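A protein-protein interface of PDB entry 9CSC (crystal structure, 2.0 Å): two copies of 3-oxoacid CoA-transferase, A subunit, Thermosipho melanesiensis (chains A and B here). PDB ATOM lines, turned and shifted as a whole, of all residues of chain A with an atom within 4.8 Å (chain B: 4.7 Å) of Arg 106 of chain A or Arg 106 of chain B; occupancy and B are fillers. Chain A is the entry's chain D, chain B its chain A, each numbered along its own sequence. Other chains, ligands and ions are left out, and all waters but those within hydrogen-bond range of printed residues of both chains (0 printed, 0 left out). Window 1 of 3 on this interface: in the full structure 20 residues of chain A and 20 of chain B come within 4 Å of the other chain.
The backbone NH of Leu 112 of chain B sits at hydrogen-bond distance from the backbone carbonyl oxygen of Ala 107 of chain B (3.0 Å). The backbone carbonyl oxygen (O) of Ala 107 of chain A sits at hydrogen-bond distance from the backbone NH (N) of Leu 112 of chain A, 3.0 Å away.
Of the printed residues of chain B, Arg 106 of chain A touches Glu 103 and Arg 106. Arg 106 of chain B touches just these residues of chain A: Glu 103 (2.9 Å) and Arg 106 (3.1 Å). Printed residues of chain B within 4 Å of Leu 112 of chain A: Glu 103. Of the printed residues of chain A, Glu 103 of chain B touches Arg 106 and Leu 112. Of the printed residues of chain B, Glu 103 of chain A touches Arg 106 and Leu 112. Of the printed residues of chain A, Leu 112 of chain B touches Glu 103 (3.7 Å). Ala 102 of chain B touches none of the printed residues of chain A. The nearest printed residue of chain B that does not touch Arg 106 of chain A is Leu 112 of chain B (6.2 Å).
NH2 of Arg 106 of chain A lies within salt-bridge range of OE2 of Glu 103 of chain B. OE1 of Glu 103 of chain A is in salt-bridge range of NH1 of Arg 106 of chain B. The guanidinium group of Arg 106 of chain A sits close to the guanidinium group of Arg 106 of chain B (3.1 Å).
Among the printed residues, pairs that only touch across the chains: Glu 103 of chain A with Leu 112 of chain B (3.7 Å) and Leu 112 of chain A with Glu 103 of chain B (3.6 Å).
Of the 12 printed residues of chain A, 3 touch a printed residue of chain B. Among the printed residues, Asp or Glu carboxylates within 4 Å of a Lys or Arg side-chain nitrogen of the other chain: Glu 103 of chain A with Arg 106 of chain B (2.9 Å) and Arg 106 of chain A with Glu 103 of chain B (2.6 Å).
Glu 103 of chain A touches Arg 106 of chain B, and with the chains exchanged Arg 106 of chain A touches Glu 103 of chain B. Glu 103 of chain A touches Leu 112 of chain B, and with the chains exchanged Leu 112 of chain A touches Glu 103 of chain B. Arg 106 of chain B touches its own counterpart, Arg 106 of chain A. Positions printed for both chains: 102, 103, 104, 105, 106, 107, 108, 109, 110, 112 and 175.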
ATOM      1  N   ALA A 102      18.681  21.145  36.825  1.00  0.00           N
ATOM      2  CA  ALA A 102      19.216  20.217  35.845  1.00  0.00           C
ATOM      3  C   ALA A 102      20.092  20.938  34.837  1.00  0.00           C
ATOM      4  O   ALA A 102      21.183  20.466  34.509  1.00  0.00           O
ATOM      5  CB  ALA A 102      18.107  19.452  35.128  1.00  0.00           C
ATOM      6  N   GLU A 103      19.616  22.074  34.307  1.00  0.00           N
ATOM      7  CA  GLU A 103      20.349  22.763  33.253  1.00  0.00           C
ATOM      8  C   GLU A 103      21.639  23.409  33.775  1.00  0.00           C
ATOM      9  O   GLU A 103      22.648  23.449  33.064  1.00  0.00           O
ATOM     10  CB  GLU A 103      19.455  23.832  32.590  1.00  0.00           C
ATOM     11  CG  GLU A 103      18.433  23.308  31.553  1.00  0.00           C
ATOM     12  CD  GLU A 103      18.984  22.261  30.564  1.00  0.00           C
ATOM     13  OE1 GLU A 103      19.931  22.569  29.815  1.00  0.00           O
ATOM     14  OE2 GLU A 103      18.456  21.105  30.571  1.00  0.00           O
ATOM     15  N   ARG A 104      21.618  23.954  34.984  1.00  0.00           N
ATOM     16  CA  ARG A 104      22.823  24.587  35.520  1.00  0.00           C
ATOM     17  C   ARG A 104      23.913  23.557  35.804  1.00  0.00           C
ATOM     18  O   ARG A 104      25.118  23.817  35.601  1.00  0.00           O
ATOM     19  CB  ARG A 104      22.477  25.372  36.803  1.00  0.00           C
ATOM     20  CG  ARG A 104      21.635  26.626  36.651  1.00  0.00           C
ATOM     21  CD  ARG A 104      21.303  27.248  37.997  1.00  0.00           C
ATOM     22  NE  ARG A 104      22.534  27.713  38.645  1.00  0.00           N
ATOM     23  CZ  ARG A 104      22.626  28.121  39.898  1.00  0.00           C
ATOM     24  NH1 ARG A 104      21.571  28.147  40.697  1.00  0.00           N
ATOM     25  NH2 ARG A 104      23.800  28.544  40.354  1.00  0.00           N
ATOM     26  N   ILE A 105      23.509  22.366  36.252  1.00  0.00           N
ATOM     27  CA  ILE A 105      24.489  21.309  36.475  1.00  0.00           C
ATOM     28  C   ILE A 105      24.999  20.811  35.137  1.00  0.00           C
ATOM     29  O   ILE A 105      26.206  20.650  34.926  1.00  0.00           O
ATOM     30  CB  ILE A 105      23.887  20.180  37.334  1.00  0.00           C
ATOM     31  CG1 ILE A 105      23.692  20.604  38.782  1.00  0.00           C
ATOM     32  CG2 ILE A 105      24.758  18.980  37.275  1.00  0.00           C
ATOM     33  CD1 ILE A 105      22.831  19.662  39.556  1.00  0.00           C
ATOM     34  N   ARG A 106      24.088  20.602  34.192  1.00  0.00           N
ATOM     35  CA  ARG A 106      24.498  20.224  32.843  1.00  0.00           C
ATOM     36  C   ARG A 106      25.396  21.276  32.218  1.00  0.00           C
ATOM     37  O   ARG A 106      26.349  20.950  31.495  1.00  0.00           O
ATOM     38  CB  ARG A 106      23.266  20.003  31.960  1.00  0.00           C
ATOM     39  CG  ARG A 106      23.570  19.987  30.449  1.00  0.00           C
ATOM     40  CD  ARG A 106      22.386  19.398  29.610  1.00  0.00           C
ATOM     41  NE  ARG A 106      22.808  18.993  28.279  1.00  0.00           N
ATOM     42  CZ  ARG A 106      23.182  19.840  27.330  1.00  0.00           C
ATOM     43  NH1 ARG A 106      23.120  21.146  27.512  1.00  0.00           N
ATOM     44  NH2 ARG A 106      23.666  19.362  26.183  1.00  0.00           N
ATOM     45  N   ALA A 107      25.120  22.549  32.466  1.00  0.00           N
ATOM     46  CA  ALA A 107      25.975  23.548  31.840  1.00  0.00           C
ATOM     47  C   ALA A 107      27.429  23.344  32.254  1.00  0.00           C
ATOM     48  O   ALA A 107      28.333  23.414  31.423  1.00  0.00           O
ATOM     49  CB  ALA A 107      25.509  24.943  32.224  1.00  0.00           C
ATOM     50  N   ALA A 108      27.665  23.087  33.534  1.00  0.00           N
ATOM     51  CA  ALA A 108      29.036  22.883  34.011  1.00  0.00           C
ATOM     52  C   ALA A 108      29.657  21.629  33.386  1.00  0.00           C
ATOM     53  O   ALA A 108      30.851  21.603  33.050  1.00  0.00           O
ATOM     54  CB  ALA A 108      29.032  22.766  35.533  1.00  0.00           C
ATOM     55  N   GLY A 109      28.855  20.575  33.210  1.00  0.00           N
ATOM     56  CA  GLY A 109      29.421  19.357  32.666  1.00  0.00           C
ATOM     57  C   GLY A 109      29.706  19.462  31.192  1.00  0.00           C
ATOM     58  O   GLY A 109      30.577  18.763  30.679  1.00  0.00           O
ATOM     59  N   VAL A 110      29.048  20.398  30.529  1.00  0.00           N
ATOM     60  CA  VAL A 110      29.058  20.531  29.097  1.00  0.00           C
ATOM     61  C   VAL A 110      29.901  21.699  28.652  1.00  0.00           C
ATOM     62  O   VAL A 110      30.119  21.873  27.448  1.00  0.00           O
ATOM     63  CB  VAL A 110      27.598  20.653  28.615  1.00  0.00           C
ATOM     64  CG1 VAL A 110      27.489  21.142  27.266  1.00  0.00           C
ATOM     65  CG2 VAL A 110      26.895  19.258  28.846  1.00  0.00           C
ATOM     66  N   GLY A 111      30.445  22.470  29.586  1.00  0.00           N
ATOM     67  CA  GLY A 111      31.275  23.605  29.213  1.00  0.00           C
ATOM     68  C   GLY A 111      30.561  24.894  28.809  1.00  0.00           C
ATOM     69  O   GLY A 111      31.192  25.772  28.251  1.00  0.00           O
ATOM     70  N   LEU A 112      29.295  25.075  29.147  1.00  0.00           N
ATOM     71  CA  LEU A 112      28.628  26.345  28.885  1.00  0.00           C
ATOM     72  C   LEU A 112      28.895  27.299  30.046  1.00  0.00           C
ATOM     73  O   LEU A 112      29.051  26.878  31.197  1.00  0.00           O
ATOM     74  CB  LEU A 112      27.131  26.143  28.739  1.00  0.00           C
ATOM     75  CG  LEU A 112      26.763  25.115  27.666  1.00  0.00           C
ATOM     76  CD1 LEU A 112      25.239  24.790  27.717  1.00  0.00           C
ATOM     77  CD2 LEU A 112      27.171  25.650  26.366  1.00  0.00           C
ATOM     78  N   ILE A 175      23.860  13.475  34.592  1.00  0.00           N
ATOM     79  CA  ILE A 175      24.247  14.862  34.409  1.00  0.00           C
ATOM     80  C   ILE A 175      25.281  15.253  35.468  1.00  0.00           C
ATOM     81  O   ILE A 175      26.275  15.910  35.157  1.00  0.00           O
ATOM     82  CB  ILE A 175      23.001  15.771  34.483  1.00  0.00           C
ATOM     83  CG1 ILE A 175      21.865  15.304  33.584  1.00  0.00           C
ATOM     84  CG2 ILE A 175      23.362  17.147  34.082  1.00  0.00           C
ATOM     85  CD1 ILE A 175      20.543  15.731  34.208  1.00  0.00           C
ATOM     86  N   ALA B 102      24.676  22.327  17.844  1.00  0.00           N
ATOM     87  CA  ALA B 102      24.027  21.345  18.694  1.00  0.00           C
ATOM     88  C   ALA B 102      23.370  22.015  19.895  1.00  0.00           C
ATOM     89  O   ALA B 102      22.244  21.675  20.244  1.00  0.00           O
ATOM     90  CB  ALA B 102      25.028  20.239  19.093  1.00  0.00           C
ATOM     91  N   GLU B 103      23.999  23.036  20.490  1.00  0.00           N
ATOM     92  CA  GLU B 103      23.361  23.621  21.664  1.00  0.00           C
ATOM     93  C   GLU B 103      22.281  24.638  21.270  1.00  0.00           C
ATOM     94  O   GLU B 103      21.242  24.716  21.935  1.00  0.00           O
ATOM     95  CB  GLU B 103      24.429  24.225  22.595  1.00  0.00           C
ATOM     96  CG  GLU B 103      25.187  23.173  23.454  1.00  0.00           C
ATOM     97  CD  GLU B 103      24.300  22.350  24.387  1.00  0.00           C
ATOM     98  OE1 GLU B 103      23.489  22.913  25.135  1.00  0.00           O
ATOM     99  OE2 GLU B 103      24.347  21.105  24.336  1.00  0.00           O
ATOM    100  N   ARG B 104      22.421  25.297  20.128  1.00  0.00           N
ATOM    101  CA  ARG B 104      21.369  26.217  19.686  1.00  0.00           C
ATOM    102  C   ARG B 104      20.090  25.465  19.307  1.00  0.00           C
ATOM    103  O   ARG B 104      18.977  25.897  19.633  1.00  0.00           O
ATOM    104  CB  ARG B 104      21.920  27.051  18.537  1.00  0.00           C
ATOM    105  CG  ARG B 104      22.915  28.133  19.001  1.00  0.00           C
ATOM    106  CD  ARG B 104      23.502  28.898  17.808  1.00  0.00           C
ATOM    107  NE  ARG B 104      22.496  29.802  17.252  1.00  0.00           N
ATOM    108  CZ  ARG B 104      22.567  30.397  16.067  1.00  0.00           C
ATOM    109  NH1 ARG B 104      23.626  30.245  15.273  1.00  0.00           N
ATOM    110  NH2 ARG B 104      21.529  31.139  15.654  1.00  0.00           N
ATOM    111  N   ILE B 105      20.225  24.311  18.674  1.00  0.00           N
ATOM    112  CA  ILE B 105      19.042  23.525  18.391  1.00  0.00           C
ATOM    113  C   ILE B 105      18.455  22.952  19.681  1.00  0.00           C
ATOM    114  O   ILE B 105      17.237  22.974  19.896  1.00  0.00           O
ATOM    115  CB  ILE B 105      19.413  22.441  17.390  1.00  0.00           C
ATOM    116  CG1 ILE B 105      19.821  23.077  16.062  1.00  0.00           C
ATOM    117  CG2 ILE B 105      18.266  21.494  17.166  1.00  0.00           C
ATOM    118  CD1 ILE B 105      20.596  22.102  15.233  1.00  0.00           C
ATOM    119  N   ARG B 106      19.309  22.452  20.570  1.00  0.00           N
ATOM    120  CA  ARG B 106      18.797  21.874  21.803  1.00  0.00           C
ATOM    121  C   ARG B 106      18.094  22.928  22.654  1.00  0.00           C
ATOM    122  O   ARG B 106      17.054  22.641  23.261  1.00  0.00           O
ATOM    123  CB  ARG B 106      19.945  21.202  22.551  1.00  0.00           C
ATOM    124  CG  ARG B 106      19.475  20.471  23.775  1.00  0.00           C
ATOM    125  CD  ARG B 106      20.644  20.091  24.722  1.00  0.00           C
ATOM    126  NE  ARG B 106      20.089  19.595  25.971  1.00  0.00           N
ATOM    127  CZ  ARG B 106      19.832  20.340  27.032  1.00  0.00           C
ATOM    128  NH1 ARG B 106      20.130  21.636  27.061  1.00  0.00           N
ATOM    129  NH2 ARG B 106      19.277  19.774  28.091  1.00  0.00           N
ATOM    130  N   ALA B 107      18.615  24.164  22.665  1.00  0.00           N
ATOM    131  CA  ALA B 107      17.969  25.233  23.417  1.00  0.00           C
ATOM    132  C   ALA B 107      16.532  25.445  22.943  1.00  0.00           C
ATOM    133  O   ALA B 107      15.632  25.695  23.747  1.00  0.00           O
ATOM    134  CB  ALA B 107      18.745  26.534  23.235  1.00  0.00           C
ATOM    135  N   ALA B 108      16.306  25.395  21.627  1.00  0.00           N
ATOM    136  CA  ALA B 108      14.940  25.509  21.122  1.00  0.00           C
ATOM    137  C   ALA B 108      14.081  24.334  21.565  1.00  0.00           C
ATOM    138  O   ALA B 108      12.900  24.504  21.905  1.00  0.00           O
ATOM    139  CB  ALA B 108      14.972  25.625  19.609  1.00  0.00           C
ATOM    140  N   GLY B 109      14.672  23.137  21.618  1.00  0.00           N
ATOM    141  CA  GLY B 109      13.897  21.962  21.956  1.00  0.00           C
ATOM    142  C   GLY B 109      13.520  21.902  23.417  1.00  0.00           C
ATOM    143  O   GLY B 109      12.450  21.379  23.762  1.00  0.00           O
ATOM    144  N   VAL B 110      14.368  22.452  24.305  1.00  0.00           N
ATOM    145  CA  VAL B 110      14.122  22.333  25.745  1.00  0.00           C
ATOM    146  C   VAL B 110      13.612  23.616  26.368  1.00  0.00           C
ATOM    147  O   VAL B 110      13.323  23.635  27.578  1.00  0.00           O
ATOM    148  CB  VAL B 110      15.357  21.815  26.512  1.00  0.00           C
ATOM    149  CG1 VAL B 110      15.735  20.471  25.893  1.00  0.00           C
ATOM    150  CG2 VAL B 110      16.482  22.813  26.443  1.00  0.00           C
ATOM    151  N   LEU B 112      14.900  26.916  26.399  1.00  0.00           N
ATOM    152  CA  LEU B 112      15.831  27.950  26.832  1.00  0.00           C
ATOM    153  C   LEU B 112      15.849  29.104  25.837  1.00  0.00           C
ATOM    154  O   LEU B 112      15.704  28.910  24.624  1.00  0.00           O
ATOM    155  CB  LEU B 112      17.259  27.404  26.943  1.00  0.00           C
ATOM    156  CG  LEU B 112      17.365  26.164  27.844  1.00  0.00           C
ATOM    157  CD1 LEU B 112      18.733  25.455  27.819  1.00  0.00           C
ATOM    158  CD2 LEU B 112      17.095  26.465  29.302  1.00  0.00           C
ATOM    159  N   ILE B 175      18.108  15.610  18.663  1.00  0.00           N
ATOM    160  CA  ILE B 175      18.086  17.015  19.062  1.00  0.00           C
ATOM    161  C   ILE B 175      17.060  17.756  18.222  1.00  0.00           C
ATOM    162  O   ILE B 175      16.239  18.533  18.734  1.00  0.00           O
ATOM    163  CB  ILE B 175      19.486  17.651  18.889  1.00  0.00           C
ATOM    164  CG1 ILE B 175      20.588  16.766  19.492  1.00  0.00           C
ATOM    165  CG2 ILE B 175      19.459  19.055  19.450  1.00  0.00           C
ATOM    166  CD1 ILE B 175      21.970  17.212  18.990  1.00  0.00           C
